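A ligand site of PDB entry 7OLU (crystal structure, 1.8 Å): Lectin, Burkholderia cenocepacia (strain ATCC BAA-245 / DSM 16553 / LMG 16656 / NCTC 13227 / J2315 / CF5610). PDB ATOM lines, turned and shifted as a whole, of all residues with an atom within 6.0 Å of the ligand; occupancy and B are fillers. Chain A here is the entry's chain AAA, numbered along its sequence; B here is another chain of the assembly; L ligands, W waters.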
ATOM      1  N   TYR A  21      17.419  -0.412  -9.236  1.00  0.00           N
ATOM      2  CA  TYR A  21      16.860  -1.608  -9.899  1.00  0.00           C
ATOM      3  C   TYR A  21      16.806  -2.728  -8.874  1.00  0.00           C
ATOM      4  O   TYR A  21      17.807  -2.997  -8.226  1.00  0.00           O
ATOM      5  CB  TYR A  21      17.641  -2.014 -11.155  1.00  0.00           C
ATOM      6  CG  TYR A  21      17.240  -1.205 -12.356  1.00  0.00           C
ATOM      7  CD1 TYR A  21      15.918  -1.252 -12.840  1.00  0.00           C
ATOM      8  CD2 TYR A  21      18.133  -0.372 -12.997  1.00  0.00           C
ATOM      9  CE1 TYR A  21      15.505  -0.504 -13.941  1.00  0.00           C
ATOM     10  CE2 TYR A  21      17.735   0.366 -14.112  1.00  0.00           C
ATOM     11  CZ  TYR A  21      16.406   0.318 -14.573  1.00  0.00           C
ATOM     12  OH  TYR A  21      16.073   1.073 -15.692  1.00  0.00           O
ATOM     13  N   PHE A  57       3.620  12.140 -11.921  1.00  0.00           N
ATOM     14  CA  PHE A  57       3.724  11.575 -13.295  1.00  0.00           C
ATOM     15  C   PHE A  57       4.300  10.186 -13.144  1.00  0.00           C
ATOM     16  O   PHE A  57       5.470   9.952 -13.445  1.00  0.00           O
ATOM     17  CB  PHE A  57       4.605  12.417 -14.217  1.00  0.00           C
ATOM     18  CG  PHE A  57       4.049  13.791 -14.452  1.00  0.00           C
ATOM     19  CD1 PHE A  57       3.155  14.015 -15.492  1.00  0.00           C
ATOM     20  CD2 PHE A  57       4.443  14.867 -13.657  1.00  0.00           C
ATOM     21  CE1 PHE A  57       2.628  15.281 -15.725  1.00  0.00           C
ATOM     22  CE2 PHE A  57       3.880  16.110 -13.887  1.00  0.00           C
ATOM     23  CZ  PHE A  57       3.016  16.315 -14.925  1.00  0.00           C
ATOM     24  N   TYR A  61      10.444   2.029 -14.482  1.00  0.00           N
ATOM     25  CA  TYR A  61      11.616   1.589 -15.280  1.00  0.00           C
ATOM     26  C   TYR A  61      11.689   0.056 -15.175  1.00  0.00           C
ATOM     27  O   TYR A  61      11.614  -0.530 -14.052  1.00  0.00           O
ATOM     28  CB  TYR A  61      12.926   2.131 -14.711  1.00  0.00           C
ATOM     29  CG  TYR A  61      13.008   3.611 -14.696  1.00  0.00           C
ATOM     30  CD1 TYR A  61      13.150   4.291 -15.887  1.00  0.00           C
ATOM     31  CD2 TYR A  61      12.932   4.340 -13.527  1.00  0.00           C
ATOM     32  CE1 TYR A  61      13.231   5.692 -15.893  1.00  0.00           C
ATOM     33  CE2 TYR A  61      12.984   5.724 -13.507  1.00  0.00           C
ATOM     34  CZ  TYR A  61      13.183   6.406 -14.705  1.00  0.00           C
ATOM     35  OH  TYR A  61      13.192   7.756 -14.667  1.00  0.00           O
ATOM     36  N   ASP A  73      17.275  -1.235 -20.887  1.00  0.00           N
ATOM     37  CA  ASP A  73      16.181  -0.737 -20.025  1.00  0.00           C
ATOM     38  C   ASP A  73      15.292   0.270 -20.745  1.00  0.00           C
ATOM     39  O   ASP A  73      15.598   0.722 -21.863  1.00  0.00           O
ATOM     40  CB  ASP A  73      16.671  -0.177 -18.682  1.00  0.00           C
ATOM     41  CG  ASP A  73      17.673   0.968 -18.706  1.00  0.00           C
ATOM     42  OD1 ASP A  73      18.110   1.349 -19.816  1.00  0.00           O
ATOM     43  OD2 ASP A  73      18.001   1.495 -17.526  1.00  0.00           O
ATOM     44  N   GLY A  74      14.143   0.498 -20.127  1.00  0.00           N
ATOM     45  CA  GLY A  74      13.137   1.458 -20.671  1.00  0.00           C
ATOM     46  C   GLY A  74      12.100   1.749 -19.644  1.00  0.00           C
ATOM     47  O   GLY A  74      12.243   1.300 -18.496  1.00  0.00           O
ATOM     48  N   CYS A  75      11.122   2.536 -20.000  1.00  0.00           N
ATOM     49  CA  CYS A  75      10.031   2.834 -19.040  1.00  0.00           C
ATOM     50  C   CYS A  75       8.748   3.190 -19.746  1.00  0.00           C
ATOM     51  O   CYS A  75       8.798   3.531 -20.948  1.00  0.00           O
ATOM     52  CB  CYS A  75      10.406   3.901 -18.040  1.00  0.00           C
ATOM     53  SG  CYS A  75      10.401   5.583 -18.703  1.00  0.00           S
ATOM     54  N   THR A  77       5.544   5.946 -18.704  1.00  0.00           N
ATOM     55  CA  THR A  77       5.084   7.013 -17.750  1.00  0.00           C
ATOM     56  C   THR A  77       3.705   7.498 -18.188  1.00  0.00           C
ATOM     57  O   THR A  77       3.388   7.440 -19.400  1.00  0.00           O
ATOM     58  CB  THR A  77       6.053   8.198 -17.651  1.00  0.00           C
ATOM     59  OG1 THR A  77       6.286   8.781 -18.920  1.00  0.00           O
ATOM     60  CG2 THR A  77       7.372   7.799 -17.056  1.00  0.00           C
ATOM     61  N   TYR A  78       2.910   7.953 -17.224  1.00  0.00           N
ATOM     62  CA  TYR A  78       1.600   8.556 -17.513  1.00  0.00           C
ATOM     63  C   TYR A  78       1.842   9.989 -17.987  1.00  0.00           C
ATOM     64  O   TYR A  78       2.941  10.498 -17.779  1.00  0.00           O
ATOM     65  CB  TYR A  78       0.684   8.476 -16.312  1.00  0.00           C
ATOM     66  CG  TYR A  78       0.367   7.060 -15.898  1.00  0.00           C
ATOM     67  CD1 TYR A  78      -0.541   6.297 -16.625  1.00  0.00           C
ATOM     68  CD2 TYR A  78       0.872   6.527 -14.727  1.00  0.00           C
ATOM     69  CE1 TYR A  78      -0.844   4.999 -16.237  1.00  0.00           C
ATOM     70  CE2 TYR A  78       0.570   5.244 -14.312  1.00  0.00           C
ATOM     71  CZ  TYR A  78      -0.320   4.490 -15.064  1.00  0.00           C
ATOM     72  OH  TYR A  78      -0.548   3.189 -14.703  1.00  0.00           O
ATOM     73  N   LYS A 111      12.432  -0.432 -11.279  1.00  0.00           N
ATOM     74  CA  LYS A 111      12.770   0.715 -10.407  1.00  0.00           C
ATOM     75  C   LYS A 111      11.689   1.770 -10.600  1.00  0.00           C
ATOM     76  O   LYS A 111      11.131   1.924 -11.720  1.00  0.00           O
ATOM     77  CB  LYS A 111      14.165   1.243 -10.765  1.00  0.00           C
ATOM     78  CG  LYS A 111      14.563   2.584 -10.181  1.00  0.00           C
ATOM     79  CD  LYS A 111      15.544   3.328 -11.078  1.00  0.00           C
ATOM     80  CE  LYS A 111      16.812   2.589 -11.339  1.00  0.00           C
ATOM     81  NZ  LYS A 111      17.638   3.369 -12.285  1.00  0.00           N
ATOM     82  N   VAL A 113       9.712   5.214 -11.095  1.00  0.00           N
ATOM     83  CA  VAL A 113       9.747   6.609 -11.609  1.00  0.00           C
ATOM     84  C   VAL A 113       9.168   7.595 -10.578  1.00  0.00           C
ATOM     85  O   VAL A 113       7.999   7.452 -10.178  1.00  0.00           O
ATOM     86  CB  VAL A 113       8.970   6.709 -12.928  1.00  0.00           C
ATOM     87  CG1 VAL A 113       8.917   8.123 -13.438  1.00  0.00           C
ATOM     88  CG2 VAL A 113       9.597   5.786 -14.008  1.00  0.00           C
ATOM     89  N   ARG A 114       9.983   8.522 -10.086  1.00  0.00           N
ATOM     90  CA  ARG A 114       9.449   9.627  -9.216  1.00  0.00           C
ATOM     91  C   ARG A 114       8.627   9.090  -8.036  1.00  0.00           C
ATOM     92  O   ARG A 114       7.509   9.600  -7.781  1.00  0.00           O
ATOM     93  CB  ARG A 114       8.665  10.569 -10.107  1.00  0.00           C
ATOM     94  CG  ARG A 114       9.550  11.478 -10.945  1.00  0.00           C
ATOM     95  CD  ARG A 114       8.822  12.439 -11.829  1.00  0.00           C
ATOM     96  NE  ARG A 114       8.024  11.791 -12.878  1.00  0.00           N
ATOM     97  CZ  ARG A 114       8.436  11.552 -14.095  1.00  0.00           C
ATOM     98  NH1 ARG A 114       9.626  11.957 -14.432  1.00  0.00           N
ATOM     99  NH2 ARG A 114       7.638  10.963 -14.985  1.00  0.00           N
ATOM    100  N   THR B  49      10.590   3.091 -25.006  1.00  0.00           N
ATOM    101  CA  THR B  49      10.517   4.372 -24.230  1.00  0.00           C
ATOM    102  C   THR B  49      10.406   5.575 -25.162  1.00  0.00           C
ATOM    103  O   THR B  49      11.037   6.575 -24.973  1.00  0.00           O
ATOM    104  CB  THR B  49      11.739   4.529 -23.287  1.00  0.00           C
ATOM    105  OG1 THR B  49      12.051   3.212 -22.772  1.00  0.00           O
ATOM    106  CG2 THR B  49      11.494   5.522 -22.165  1.00  0.00           C
ATOM    107  N   TYR B  51       8.647   8.994 -27.019  1.00  0.00           N
ATOM    108  CA  TYR B  51       7.565   9.984 -26.815  1.00  0.00           C
ATOM    109  C   TYR B  51       7.433  10.846 -28.040  1.00  0.00           C
ATOM    110  O   TYR B  51       8.290  10.832 -28.860  1.00  0.00           O
ATOM    111  CB  TYR B  51       7.720  10.727 -25.512  1.00  0.00           C
ATOM    112  CG  TYR B  51       8.844  11.729 -25.492  1.00  0.00           C
ATOM    113  CD1 TYR B  51      10.134  11.343 -25.157  1.00  0.00           C
ATOM    114  CD2 TYR B  51       8.602  13.073 -25.664  1.00  0.00           C
ATOM    115  CE1 TYR B  51      11.159  12.261 -25.050  1.00  0.00           C
ATOM    116  CE2 TYR B  51       9.620  14.008 -25.521  1.00  0.00           C
ATOM    117  CZ  TYR B  51      10.917  13.605 -25.222  1.00  0.00           C
ATOM    118  OH  TYR B  51      11.943  14.528 -25.070  1.00  0.00           O
ATOM    119  N   TYR B  78      -1.440   9.731 -28.057  1.00  0.00           N
ATOM    120  CA  TYR B  78      -1.941  10.180 -26.756  1.00  0.00           C
ATOM    121  C   TYR B  78      -3.446  10.380 -26.875  1.00  0.00           C
ATOM    122  O   TYR B  78      -3.944  10.443 -27.988  1.00  0.00           O
ATOM    123  CB  TYR B  78      -1.206  11.432 -26.296  1.00  0.00           C
ATOM    124  CG  TYR B  78       0.273  11.218 -26.091  1.00  0.00           C
ATOM    125  CD1 TYR B  78       0.735  10.539 -24.962  1.00  0.00           C
ATOM    126  CD2 TYR B  78       1.198  11.782 -26.938  1.00  0.00           C
ATOM    127  CE1 TYR B  78       2.101  10.356 -24.759  1.00  0.00           C
ATOM    128  CE2 TYR B  78       2.563  11.625 -26.743  1.00  0.00           C
ATOM    129  CZ  TYR B  78       3.007  10.932 -25.635  1.00  0.00           C
ATOM    130  OH  TYR B  78       4.350  10.699 -25.499  1.00  0.00           O
ATOM    131  N   SER B  85       2.042  16.287 -19.850  1.00  0.00           N
ATOM    132  CA  SER B  85       3.425  15.849 -20.033  1.00  0.00           C
ATOM    133  C   SER B  85       3.383  14.653 -21.006  1.00  0.00           C
ATOM    134  O   SER B  85       2.558  13.867 -20.918  1.00  0.00           O
ATOM    135  CB  SER B  85       4.057  15.479 -18.701  1.00  0.00           C
ATOM    136  OG  SER B  85       5.234  14.717 -18.923  1.00  0.00           O
ATOM    137  N   THR B  86       4.175  14.673 -22.035  1.00  0.00           N
ATOM    138  CA  THR B  86       4.178  13.571 -23.048  1.00  0.00           C
ATOM    139  C   THR B  86       4.875  12.355 -22.409  1.00  0.00           C
ATOM    140  O   THR B  86       6.127  12.260 -22.470  1.00  0.00           O
ATOM    141  CB  THR B  86       4.779  14.093 -24.342  1.00  0.00           C
ATOM    142  OG1 THR B  86       6.077  14.578 -24.078  1.00  0.00           O
ATOM    143  CG2 THR B  86       3.940  15.160 -25.014  1.00  0.00           C
ATOM    144  N   GLY B  87       4.083  11.411 -21.950  1.00  0.00           N
ATOM    145  CA  GLY B  87       4.648  10.249 -21.249  1.00  0.00           C
ATOM    146  C   GLY B  87       5.247   9.242 -22.199  1.00  0.00           C
ATOM    147  O   GLY B  87       4.995   9.304 -23.420  1.00  0.00           O
ATOM    148  N   ARG B  88       6.074   8.359 -21.658  1.00  0.00           N
ATOM    149  CA  ARG B  88       6.742   7.305 -22.450  1.00  0.00           C
ATOM    150  C   ARG B  88       5.732   6.214 -22.808  1.00  0.00           C
ATOM    151  O   ARG B  88       5.104   5.671 -21.896  1.00  0.00           O
ATOM    152  CB  ARG B  88       7.991   6.806 -21.751  1.00  0.00           C
ATOM    153  CG  ARG B  88       8.989   7.912 -21.416  1.00  0.00           C
ATOM    154  CD  ARG B  88       9.346   8.770 -22.593  1.00  0.00           C
ATOM    155  NE  ARG B  88      10.400   9.715 -22.238  1.00  0.00           N
ATOM    156  CZ  ARG B  88      11.618   9.755 -22.677  1.00  0.00           C
ATOM    157  NH1 ARG B  88      12.068   8.891 -23.562  1.00  0.00           N
ATOM    158  NH2 ARG B  88      12.416  10.749 -22.254  1.00  0.00           N
ATOM    159  N   ASP B 121      15.336   8.532 -27.076  1.00  0.00           N
ATOM    160  CA  ASP B 121      16.515   9.075 -26.346  1.00  0.00           C
ATOM    161  C   ASP B 121      17.103   7.984 -25.422  1.00  0.00           C
ATOM    162  O   ASP B 121      17.822   8.313 -24.473  1.00  0.00           O
ATOM    163  CB  ASP B 121      16.113  10.345 -25.647  1.00  0.00           C
ATOM    164  CG  ASP B 121      15.139  10.165 -24.502  1.00  0.00           C
ATOM    165  OD1 ASP B 121      14.727   9.010 -24.290  1.00  0.00           O
ATOM    166  OD2 ASP B 121      14.733  11.196 -23.894  1.00  0.00           O
ATOM    167  N   SER B 122      16.796   6.726 -25.676  1.00  0.00           N
ATOM    168  CA  SER B 122      17.279   5.615 -24.859  1.00  0.00           C
ATOM    169  C   SER B 122      17.266   4.328 -25.690  1.00  0.00           C
ATOM    170  O   SER B 122      16.856   4.376 -26.875  1.00  0.00           O
ATOM    171  CB  SER B 122      16.459   5.487 -23.580  1.00  0.00           C
ATOM    172  OG  SER B 122      15.122   5.256 -23.853  1.00  0.00           O
ATOM    173  N   TYR B 123      17.527   3.209 -25.037  1.00  0.00           N
ATOM    174  CA  TYR B 123      17.601   1.890 -25.688  1.00  0.00           C
ATOM    175  C   TYR B 123      16.368   1.639 -26.600  1.00  0.00           C
ATOM    176  O   TYR B 123      15.193   1.776 -26.194  1.00  0.00           O
ATOM    177  CB  TYR B 123      17.692   0.815 -24.612  1.00  0.00           C
ATOM    178  CG  TYR B 123      17.810  -0.565 -25.200  1.00  0.00           C
ATOM    179  CD1 TYR B 123      16.674  -1.277 -25.519  1.00  0.00           C
ATOM    180  CD2 TYR B 123      19.027  -1.115 -25.513  1.00  0.00           C
ATOM    181  CE1 TYR B 123      16.743  -2.557 -26.031  1.00  0.00           C
ATOM    182  CE2 TYR B 123      19.102  -2.363 -26.093  1.00  0.00           C
ATOM    183  CZ  TYR B 123      17.951  -3.096 -26.353  1.00  0.00           C
ATOM    184  OH  TYR B 123      18.012  -4.311 -26.944  1.00  0.00           O
HETATM  185  N1  LIG L   1      18.377   6.249 -19.162  1.00  0.00           N
HETATM  186  C1  LIG L   1       8.277  12.331 -19.896  1.00  0.00           C
HETATM  187  C2  LIG L   1       9.530  13.022 -20.379  1.00  0.00           C
HETATM  188  C3  LIG L   1       9.440  13.483 -21.808  1.00  0.00           C
HETATM  189  C4  LIG L   1      12.019  10.660 -19.043  1.00  0.00           C
HETATM  190  C5  LIG L   1      12.852   9.816 -19.041  1.00  0.00           C
HETATM  191  C6  LIG L   1      14.524   8.389 -17.936  1.00  0.00           C
HETATM  192  C7  LIG L   1      14.572   6.752 -20.180  1.00  0.00           C
HETATM  193  C8  LIG L   1      16.233   5.111 -19.149  1.00  0.00           C
HETATM  194  C9  LIG L   1      15.524   3.966 -19.889  1.00  0.00           C
HETATM  195  O1  LIG L   1      10.627  12.093 -20.316  1.00  0.00           O
HETATM  196  C10 LIG L   1       8.499  11.822 -18.483  1.00  0.00           C
HETATM  197  C11 LIG L   1       9.695  10.943 -18.363  1.00  0.00           C
HETATM  198  C12 LIG L   1      10.918  11.623 -18.984  1.00  0.00           C
HETATM  199  O2  LIG L   1       9.924  10.610 -17.003  1.00  0.00           O
HETATM  200  O3  LIG L   1       7.332  11.111 -18.034  1.00  0.00           O
HETATM  201  O4  LIG L   1       7.994  11.276 -20.818  1.00  0.00           O
HETATM  202  C13 LIG L   1      13.744   8.701 -19.049  1.00  0.00           C
HETATM  203  C14 LIG L   1      15.324   7.244 -17.950  1.00  0.00           C
HETATM  204  C15 LIG L   1      15.361   6.386 -19.075  1.00  0.00           C
HETATM  205  C16 LIG L   1      13.795   7.874 -20.169  1.00  0.00           C
HETATM  206  C17 LIG L   1      17.479   5.445 -19.985  1.00  0.00           C
HETATM  207  C18 LIG L   1      16.583   4.612 -17.750  1.00  0.00           C
HETATM  208  O   HOH W   1      11.146   8.208 -16.449  1.00  0.00           O
HETATM  209  O   HOH W   2      16.449   4.235 -14.567  1.00  0.00           O
HETATM  210  O   HOH W   3       4.928  12.226 -18.067  1.00  0.00           O
HETATM  211  O   HOH W   4      19.841   3.507 -20.018  1.00  0.00           O
HETATM  212  O   HOH W   5      13.675  13.198 -20.309  1.00  0.00           O
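O4 of the ligand is in hydrogen-bond range of O of Thr 86 of chain B, 2.7 Å away. An oxygen (O3) of the ligand sits at hydrogen-bond distance from the side-chain hydroxyl (OG1) of Thr 77 (2.7 Å). An oxygen (O2) of the ligand is in hydrogen-bond range of the guanidinium group (NH1) of Arg 114, 2.9 Å away. NH2 of Arg 88 of chain B is in hydrogen-bond range of O1 of the ligand, 3.0 Å away.
Tyr 61 touches the ligand. Asp 73 touches the ligand (OD2 to C18, 3.4 Å). CA of Gly 74 touches C9 of the ligand, at 3.5 Å. CG2 of Thr 49 of chain B touches C16 of the ligand, 3.8 Å away. Tyr 51 of chain B touches the ligand (CZ to C3, 3.7 Å). Ser 85 of chain B touches the ligand (OG to C1, 3.99 Å). Gly 87 of chain B touches the ligand. Ser 122 of chain B touches the ligand (CB to C17, 3.7 Å). Within 4 Å of the ligand: Tyr 61, Asp 73, Gly 74, Thr 77, Arg 114, Thr 49 of chain B, Tyr 51 of chain B, Ser 85 of chain B, Thr 86 of chain B, Gly 87 of chain B, Arg 88 of chain B and Ser 122 of chain B.
Water W3 lies within hydrogen-bond range of O of Tyr 78 of chain A (2.6 Å), O3 of the ligand (2.7 Å) and OG of Ser 85 of chain B (2.7 Å). Water W1 lies within hydrogen-bond range of OH of Tyr 61 (2.8 Å), O2 of the ligand (2.8 Å) and SG of Cys 75 (3.5 Å). Water W4 lies within hydrogen-bond range of the side-chain carboxylate of Asp 73 (2.8 Å) and a nitrogen (N1) of the ligand (3.2 Å). Water W2 bridges NZ of Lys 111 (2.7 Å) and OH of Tyr 21 (3.4 Å). Water W5 lies within hydrogen-bond range of O1 of the ligand (3.2 Å) and NH2 of Arg 88 of chain B (3.4 Å).
OG1 of Thr 77 sits at hydrogen-bond distance from N of Arg 88 of chain B (2.8 Å). The guanidinium group (NH2) of Arg 114 lies within hydrogen-bond range of the backbone carbonyl oxygen (O) of Phe 57, at 2.8 Å. The backbone carbonyl oxygen (O) of Thr 49 of chain B lies within hydrogen-bond range of the guanidinium group (NH1) of Arg 88 of chain B (2.9 Å). The guanidinium group of Arg 88 of chain B lies within salt-bridge range of the side-chain carboxylate of Asp 121 of chain B, at 2.8 Å. The backbone NH (N) of Tyr 61 is in hydrogen-bond range of the backbone carbonyl oxygen (O) of Lys 111 (2.8 Å). The side-chain carboxylate (OD2) of Asp 73 sits at hydrogen-bond distance from the side-chain hydroxyl (OH) of Tyr 21 (2.7 Å). O of Gly 87 of chain B lies within hydrogen-bond range of OH of Tyr 78 of chain B. OG1 of Thr 49 of chain B lies within hydrogen-bond range of N of Cys 75.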
